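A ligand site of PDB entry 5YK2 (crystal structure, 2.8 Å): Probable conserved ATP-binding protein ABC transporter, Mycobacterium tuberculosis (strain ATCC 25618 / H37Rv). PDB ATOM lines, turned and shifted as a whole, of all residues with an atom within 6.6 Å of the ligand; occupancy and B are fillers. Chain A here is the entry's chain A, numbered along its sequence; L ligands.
The side-chain carboxylate of Glu 201 is in hydrogen-bond range of an oxygen (O8) of the ligand. NH2 of Arg 415 lies within hydrogen-bond range of O3 of the ligand, at 3.1 Å. N of Asp 291 sits at hydrogen-bond distance from O7 of the ligand (3.4 Å). O7 of the ligand is in hydrogen-bond range of OD1 of Asp 291, at 3.2 Å.
The side-chain carboxylate (OE2) of Glu 201 is in salt-bridge range of the guanidinium group (NE) of Arg 205. N of Gly 290 lies close to O of Ala 312, 3.3 Å away. The backbone NH (N) of Met 288 lies within hydrogen-bond range of the backbone carbonyl oxygen (O) of Ala 314 (2.9 Å).
Residues that only touch the ligand: Glu 204, Arg 205, Gly 290, Gly 311, Ala 312, Ala 314, Pro 315, Ile 412 and Val 416.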
ATOM      1  N   GLY A 197     -12.636  11.930  27.062  1.00  0.00           N
ATOM      2  CA  GLY A 197     -12.495  11.171  25.832  1.00  0.00           C
ATOM      3  C   GLY A 197     -12.664   9.665  25.963  1.00  0.00           C
ATOM      4  O   GLY A 197     -12.547   8.934  24.986  1.00  0.00           O
ATOM      5  N   ASP A 200     -15.707   8.913  24.056  1.00  0.00           N
ATOM      6  CA  ASP A 200     -15.373   9.033  22.639  1.00  0.00           C
ATOM      7  C   ASP A 200     -14.602   7.822  22.152  1.00  0.00           C
ATOM      8  O   ASP A 200     -14.818   7.339  21.040  1.00  0.00           O
ATOM      9  CB  ASP A 200     -14.567  10.305  22.378  1.00  0.00           C
ATOM     10  CG  ASP A 200     -15.369  11.569  22.623  1.00  0.00           C
ATOM     11  OD1 ASP A 200     -16.613  11.489  22.629  1.00  0.00           O
ATOM     12  OD2 ASP A 200     -14.752  12.642  22.803  1.00  0.00           O
ATOM     13  N   GLU A 201     -13.694   7.325  22.990  1.00  0.00           N
ATOM     14  CA  GLU A 201     -12.910   6.133  22.678  1.00  0.00           C
ATOM     15  C   GLU A 201     -13.816   4.921  22.528  1.00  0.00           C
ATOM     16  O   GLU A 201     -13.733   4.190  21.539  1.00  0.00           O
ATOM     17  CB  GLU A 201     -11.867   5.886  23.763  1.00  0.00           C
ATOM     18  CG  GLU A 201     -10.916   4.732  23.481  1.00  0.00           C
ATOM     19  CD  GLU A 201      -9.810   5.118  22.510  1.00  0.00           C
ATOM     20  OE1 GLU A 201      -9.579   6.325  22.326  1.00  0.00           O
ATOM     21  OE2 GLU A 201      -9.162   4.206  21.956  1.00  0.00           O
ATOM     22  N   LEU A 202     -14.680   4.703  23.517  1.00  0.00           N
ATOM     23  CA  LEU A 202     -15.564   3.539  23.534  1.00  0.00           C
ATOM     24  C   LEU A 202     -16.579   3.547  22.400  1.00  0.00           C
ATOM     25  O   LEU A 202     -16.886   2.506  21.826  1.00  0.00           O
ATOM     26  CB  LEU A 202     -16.290   3.462  24.886  1.00  0.00           C
ATOM     27  CG  LEU A 202     -15.421   3.116  26.094  1.00  0.00           C
ATOM     28  CD1 LEU A 202     -16.229   3.173  27.379  1.00  0.00           C
ATOM     29  CD2 LEU A 202     -14.793   1.746  25.917  1.00  0.00           C
ATOM     30  N   GLU A 204     -16.178   5.015  19.494  1.00  0.00           N
ATOM     31  CA  GLU A 204     -15.442   4.787  18.253  1.00  0.00           C
ATOM     32  C   GLU A 204     -15.055   3.323  18.102  1.00  0.00           C
ATOM     33  O   GLU A 204     -15.235   2.737  17.031  1.00  0.00           O
ATOM     34  CB  GLU A 204     -14.201   5.670  18.191  1.00  0.00           C
ATOM     35  CG  GLU A 204     -13.850   6.145  16.793  1.00  0.00           C
ATOM     36  CD  GLU A 204     -14.973   6.925  16.139  1.00  0.00           C
ATOM     37  OE1 GLU A 204     -15.151   6.802  14.907  1.00  0.00           O
ATOM     38  OE2 GLU A 204     -15.686   7.664  16.855  1.00  0.00           O
ATOM     39  N   ARG A 205     -14.538   2.727  19.173  1.00  0.00           N
ATOM     40  CA  ARG A 205     -14.161   1.321  19.172  1.00  0.00           C
ATOM     41  C   ARG A 205     -15.344   0.419  18.834  1.00  0.00           C
ATOM     42  O   ARG A 205     -15.205  -0.529  18.059  1.00  0.00           O
ATOM     43  CB  ARG A 205     -13.594   0.897  20.524  1.00  0.00           C
ATOM     44  CG  ARG A 205     -12.232   1.471  20.867  1.00  0.00           C
ATOM     45  CD  ARG A 205     -11.692   0.794  22.126  1.00  0.00           C
ATOM     46  NE  ARG A 205     -10.463   1.413  22.608  1.00  0.00           N
ATOM     47  CZ  ARG A 205      -9.715   0.918  23.582  1.00  0.00           C
ATOM     48  NH1 ARG A 205      -8.608   1.542  23.962  1.00  0.00           N
ATOM     49  NH2 ARG A 205     -10.062  -0.223  24.161  1.00  0.00           N
ATOM     50  N   THR A 206     -16.491   0.728  19.417  1.00  0.00           N
ATOM     51  CA  THR A 206     -17.674  -0.126  19.314  1.00  0.00           C
ATOM     52  C   THR A 206     -18.168  -0.303  17.888  1.00  0.00           C
ATOM     53  O   THR A 206     -18.350  -1.437  17.426  1.00  0.00           O
ATOM     54  CB  THR A 206     -18.822   0.418  20.186  1.00  0.00           C
ATOM     55  OG1 THR A 206     -18.443   0.370  21.571  1.00  0.00           O
ATOM     56  CG2 THR A 206     -20.077  -0.415  19.991  1.00  0.00           C
ATOM     57  N   MET A 208     -16.637   0.554  15.130  1.00  0.00           N
ATOM     58  CA  MET A 208     -15.566   0.059  14.270  1.00  0.00           C
ATOM     59  C   MET A 208     -15.628  -1.474  14.261  1.00  0.00           C
ATOM     60  O   MET A 208     -15.211  -2.113  13.299  1.00  0.00           O
ATOM     61  CB  MET A 208     -14.194   0.541  14.740  1.00  0.00           C
ATOM     62  CG  MET A 208     -13.854   1.967  14.310  1.00  0.00           C
ATOM     63  SD  MET A 208     -13.898   2.189  12.519  1.00  0.00           S
ATOM     64  CE  MET A 208     -12.758   0.928  11.980  1.00  0.00           C
ATOM     65  N   MET A 288      -1.770   5.946   8.561  1.00  0.00           N
ATOM     66  CA  MET A 288      -0.860   4.975   9.153  1.00  0.00           C
ATOM     67  C   MET A 288      -1.624   3.754   9.632  1.00  0.00           C
ATOM     68  O   MET A 288      -2.551   3.881  10.436  1.00  0.00           O
ATOM     69  CB  MET A 288      -0.066   5.602  10.299  1.00  0.00           C
ATOM     70  CG  MET A 288       1.155   4.789  10.701  1.00  0.00           C
ATOM     71  SD  MET A 288       2.267   5.677  11.813  1.00  0.00           S
ATOM     72  CE  MET A 288       2.601   7.151  10.852  1.00  0.00           C
ATOM     73  N   HIS A 289      -1.247   2.589   9.126  1.00  0.00           N
ATOM     74  CA  HIS A 289      -1.816   1.322   9.587  1.00  0.00           C
ATOM     75  C   HIS A 289      -1.592   1.230  11.094  1.00  0.00           C
ATOM     76  O   HIS A 289      -0.464   1.306  11.566  1.00  0.00           O
ATOM     77  CB  HIS A 289      -1.169   0.141   8.866  1.00  0.00           C
ATOM     78  CG  HIS A 289      -1.837  -1.171   9.137  1.00  0.00           C
ATOM     79  ND1 HIS A 289      -1.384  -2.053  10.085  1.00  0.00           N
ATOM     80  CD2 HIS A 289      -2.920  -1.761   8.566  1.00  0.00           C
ATOM     81  CE1 HIS A 289      -2.159  -3.119  10.109  1.00  0.00           C
ATOM     82  NE2 HIS A 289      -3.099  -2.963   9.190  1.00  0.00           N
ATOM     83  N   GLY A 290      -2.687   1.077  11.843  1.00  0.00           N
ATOM     84  CA  GLY A 290      -2.639   1.123  13.291  1.00  0.00           C
ATOM     85  C   GLY A 290      -1.813   0.038  13.935  1.00  0.00           C
ATOM     86  O   GLY A 290      -1.120  -0.711  13.255  1.00  0.00           O
ATOM     87  N   ASP A 291      -1.893  -0.049  15.272  1.00  0.00           N
ATOM     88  CA  ASP A 291      -1.143  -1.034  16.031  1.00  0.00           C
ATOM     89  C   ASP A 291      -1.304  -2.422  15.436  1.00  0.00           C
ATOM     90  O   ASP A 291      -2.409  -2.973  15.372  1.00  0.00           O
ATOM     91  CB  ASP A 291      -1.576  -1.028  17.498  1.00  0.00           C
ATOM     92  CG  ASP A 291      -0.992   0.136  18.267  1.00  0.00           C
ATOM     93  OD1 ASP A 291      -1.568   1.239  18.201  1.00  0.00           O
ATOM     94  OD2 ASP A 291       0.049  -0.049  18.943  1.00  0.00           O
ATOM     95  N   GLY A 311      -8.816  -2.328  10.427  1.00  0.00           N
ATOM     96  CA  GLY A 311      -9.760  -1.791  11.387  1.00  0.00           C
ATOM     97  C   GLY A 311      -9.089  -0.911  12.430  1.00  0.00           C
ATOM     98  O   GLY A 311      -9.690  -0.593  13.460  1.00  0.00           O
ATOM     99  N   ALA A 312      -7.855  -0.518  12.168  1.00  0.00           N
ATOM    100  CA  ALA A 312      -7.091   0.260  13.139  1.00  0.00           C
ATOM    101  C   ALA A 312      -6.378   1.459  12.523  1.00  0.00           C
ATOM    102  O   ALA A 312      -5.538   2.082  13.172  1.00  0.00           O
ATOM    103  CB  ALA A 312      -6.087  -0.643  13.839  1.00  0.00           C
ATOM    104  N   VAL A 313      -6.714   1.788  11.283  1.00  0.00           N
ATOM    105  CA  VAL A 313      -6.045   2.875  10.565  1.00  0.00           C
ATOM    106  C   VAL A 313      -6.187   4.221  11.285  1.00  0.00           C
ATOM    107  O   VAL A 313      -7.291   4.646  11.626  1.00  0.00           O
ATOM    108  CB  VAL A 313      -6.592   3.017   9.130  1.00  0.00           C
ATOM    109  CG1 VAL A 313      -5.889   4.148   8.399  1.00  0.00           C
ATOM    110  CG2 VAL A 313      -6.434   1.705   8.374  1.00  0.00           C
ATOM    111  N   ALA A 314      -5.061   4.889  11.493  1.00  0.00           N
ATOM    112  CA  ALA A 314      -5.035   6.214  12.108  1.00  0.00           C
ATOM    113  C   ALA A 314      -4.691   7.282  11.073  1.00  0.00           C
ATOM    114  O   ALA A 314      -3.875   7.057  10.182  1.00  0.00           O
ATOM    115  CB  ALA A 314      -4.038   6.242  13.253  1.00  0.00           C
ATOM    116  N   PRO A 315      -5.329   8.462  11.188  1.00  0.00           N
ATOM    117  CA  PRO A 315      -5.108   9.543  10.224  1.00  0.00           C
ATOM    118  C   PRO A 315      -3.771  10.278  10.408  1.00  0.00           C
ATOM    119  O   PRO A 315      -3.440  10.694  11.516  1.00  0.00           O
ATOM    120  CB  PRO A 315      -6.282  10.490  10.491  1.00  0.00           C
ATOM    121  CG  PRO A 315      -6.606  10.269  11.923  1.00  0.00           C
ATOM    122  CD  PRO A 315      -6.341   8.812  12.187  1.00  0.00           C
ATOM    123  N   ALA A 408      -0.986  14.689  19.472  1.00  0.00           N
ATOM    124  CA  ALA A 408      -1.532  13.569  18.714  1.00  0.00           C
ATOM    125  C   ALA A 408      -0.666  13.162  17.523  1.00  0.00           C
ATOM    126  O   ALA A 408      -0.521  11.967  17.230  1.00  0.00           O
ATOM    127  CB  ALA A 408      -2.941  13.899  18.229  1.00  0.00           C
ATOM    128  N   ALA A 411       2.211  11.297  19.072  1.00  0.00           N
ATOM    129  CA  ALA A 411       1.794  10.138  19.849  1.00  0.00           C
ATOM    130  C   ALA A 411       1.418   8.960  18.945  1.00  0.00           C
ATOM    131  O   ALA A 411       1.752   7.818  19.244  1.00  0.00           O
ATOM    132  CB  ALA A 411       0.631  10.500  20.751  1.00  0.00           C
ATOM    133  N   ILE A 412       0.722   9.254  17.858  1.00  0.00           N
ATOM    134  CA  ILE A 412       0.260   8.207  16.938  1.00  0.00           C
ATOM    135  C   ILE A 412       1.403   7.405  16.310  1.00  0.00           C
ATOM    136  O   ILE A 412       1.396   6.178  16.392  1.00  0.00           O
ATOM    137  CB  ILE A 412      -0.628   8.802  15.818  1.00  0.00           C
ATOM    138  CG1 ILE A 412      -1.967   9.271  16.393  1.00  0.00           C
ATOM    139  CG2 ILE A 412      -0.862   7.784  14.722  1.00  0.00           C
ATOM    140  CD1 ILE A 412      -2.903   9.866  15.371  1.00  0.00           C
ATOM    141  N   PRO A 413       2.391   8.065  15.684  1.00  0.00           N
ATOM    142  CA  PRO A 413       3.416   7.236  15.040  1.00  0.00           C
ATOM    143  C   PRO A 413       4.355   6.538  16.032  1.00  0.00           C
ATOM    144  O   PRO A 413       4.760   5.399  15.774  1.00  0.00           O
ATOM    145  CB  PRO A 413       4.191   8.233  14.178  1.00  0.00           C
ATOM    146  CG  PRO A 413       4.042   9.529  14.892  1.00  0.00           C
ATOM    147  CD  PRO A 413       2.665   9.503  15.482  1.00  0.00           C
ATOM    148  N   ARG A 415       3.746   5.316  18.986  1.00  0.00           N
ATOM    149  CA  ARG A 415       3.112   4.112  19.506  1.00  0.00           C
ATOM    150  C   ARG A 415       3.173   2.986  18.485  1.00  0.00           C
ATOM    151  O   ARG A 415       3.449   1.839  18.831  1.00  0.00           O
ATOM    152  CB  ARG A 415       1.658   4.392  19.902  1.00  0.00           C
ATOM    153  CG  ARG A 415       1.492   5.276  21.110  1.00  0.00           C
ATOM    154  CD  ARG A 415       0.023   5.586  21.353  1.00  0.00           C
ATOM    155  NE  ARG A 415      -0.163   6.647  22.334  1.00  0.00           N
ATOM    156  CZ  ARG A 415      -1.345   7.175  22.635  1.00  0.00           C
ATOM    157  NH1 ARG A 415      -1.428   8.139  23.537  1.00  0.00           N
ATOM    158  NH2 ARG A 415      -2.447   6.731  22.041  1.00  0.00           N
ATOM    159  N   VAL A 416       2.903   3.325  17.229  1.00  0.00           N
ATOM    160  CA  VAL A 416       2.932   2.351  16.151  1.00  0.00           C
ATOM    161  C   VAL A 416       4.345   1.793  15.951  1.00  0.00           C
ATOM    162  O   VAL A 416       4.526   0.580  15.856  1.00  0.00           O
ATOM    163  CB  VAL A 416       2.434   2.966  14.827  1.00  0.00           C
ATOM    164  CG1 VAL A 416       2.656   2.002  13.666  1.00  0.00           C
ATOM    165  CG2 VAL A 416       0.966   3.345  14.928  1.00  0.00           C
HETATM  166  C1  LIG L   1      -7.717   2.656  17.178  1.00  0.00           C
HETATM  167  C2  LIG L   1      -6.281   2.534  17.721  1.00  0.00           C
HETATM  168  C3  LIG L   1      -5.155   3.149  16.859  1.00  0.00           C
HETATM  169  C4  LIG L   1      -4.321   4.077  17.750  1.00  0.00           C
HETATM  170  O1  LIG L   1      -4.945   5.393  17.741  1.00  0.00           O
HETATM  171  C5  LIG L   1      -4.900   7.648  18.438  1.00  0.00           C
HETATM  172  C6  LIG L   1      -6.402   8.040  18.567  1.00  0.00           C
HETATM  173  C7  LIG L   1      -7.234   7.238  17.550  1.00  0.00           C
HETATM  174  C8  LIG L   1      -8.757   7.342  17.826  1.00  0.00           C
HETATM  175  C9  LIG L   1      -9.309   6.065  18.475  1.00  0.00           C
HETATM  176  C10 LIG L   1      -9.593   4.961  17.453  1.00  0.00           C
HETATM  177  C11 LIG L   1      -9.973   3.611  18.070  1.00  0.00           C
HETATM  178  C12 LIG L   1      -8.790   2.669  18.246  1.00  0.00           C
HETATM  179  O2  LIG L   1      -8.682   1.978  19.235  1.00  0.00           O
HETATM  180  C13 LIG L   1      -4.714   6.180  18.771  1.00  0.00           C
HETATM  181  O3  LIG L   1      -4.375   5.784  19.844  1.00  0.00           O
HETATM  182  O4  LIG L   1      -6.626   9.439  18.342  1.00  0.00           O
HETATM  183  O5  LIG L   1      -9.504   7.519  16.605  1.00  0.00           O
HETATM  184  C14 LIG L   1      -8.106   1.579  16.178  1.00  0.00           C
HETATM  185  C15 LIG L   1     -10.988   2.943  17.162  1.00  0.00           C
HETATM  186  C16 LIG L   1      -5.701   3.934  15.734  1.00  0.00           C
HETATM  187  O6  LIG L   1      -5.933   1.176  17.905  1.00  0.00           O
HETATM  188  O7  LIG L   1      -4.071   2.209  16.548  1.00  0.00           O
HETATM  189  C17 LIG L   1      -2.883   4.259  17.282  1.00  0.00           C
HETATM  190  C18 LIG L   1      -4.002   8.480  19.335  1.00  0.00           C
HETATM  191  C19 LIG L   1     -10.565   6.389  19.276  1.00  0.00           C
HETATM  192  O8  LIG L   1      -8.309   5.537  19.357  1.00  0.00           O
HETATM  193  C20 LIG L   1     -10.188   8.712  16.410  1.00  0.00           C
HETATM  194  C21 LIG L   1     -10.723   8.729  14.990  1.00  0.00           C
HETATM  195  C22 LIG L   1     -11.507  10.007  14.796  1.00  0.00           C
HETATM  196  C23 LIG L   1     -12.617  10.080  15.833  1.00  0.00           C
HETATM  197  C24 LIG L   1     -12.012  10.009  17.210  1.00  0.00           C
HETATM  198  O9  LIG L   1     -11.249   8.798  17.329  1.00  0.00           O
HETATM  199  N1  LIG L   1     -11.857  10.214  13.389  1.00  0.00           N
HETATM  200  C25 LIG L   1     -13.040   9.981  18.308  1.00  0.00           C
HETATM  201  O10 LIG L   1      -9.636   8.687  14.074  1.00  0.00           O
HETATM  202  C26 LIG L   1     -12.996  11.103  13.202  1.00  0.00           C
HETATM  203  C27 LIG L   1      -6.699  10.250  19.487  1.00  0.00           C
HETATM  204  C28 LIG L   1      -6.367  11.667  19.099  1.00  0.00           C
HETATM  205  C29 LIG L   1      -7.484  12.398  18.386  1.00  0.00           C
HETATM  206  C30 LIG L   1      -8.755  12.232  19.202  1.00  0.00           C
HETATM  207  C31 LIG L   1      -9.051  10.781  19.489  1.00  0.00           C
HETATM  208  O11 LIG L   1      -7.936  10.156  20.159  1.00  0.00           O
HETATM  209  O12 LIG L   1      -7.803  11.818  17.112  1.00  0.00           O
HETATM  210  O13 LIG L   1      -9.847  12.778  18.508  1.00  0.00           O
HETATM  211  C32 LIG L   1      -6.918  12.045  16.029  1.00  0.00           C
HETATM  212  C33 LIG L   1     -10.725  10.682  12.603  1.00  0.00           C
HETATM  213  C34 LIG L   1     -10.201  10.621  20.439  1.00  0.00           C
HETATM  214  C35 LIG L   1      -2.558   4.888  15.990  1.00  0.00           C
HETATM  215  C36 LIG L   1      -6.845   7.589  16.122  1.00  0.00           C
HETATM  216  C37 LIG L   1      -7.133  13.856  18.229  1.00  0.00           C
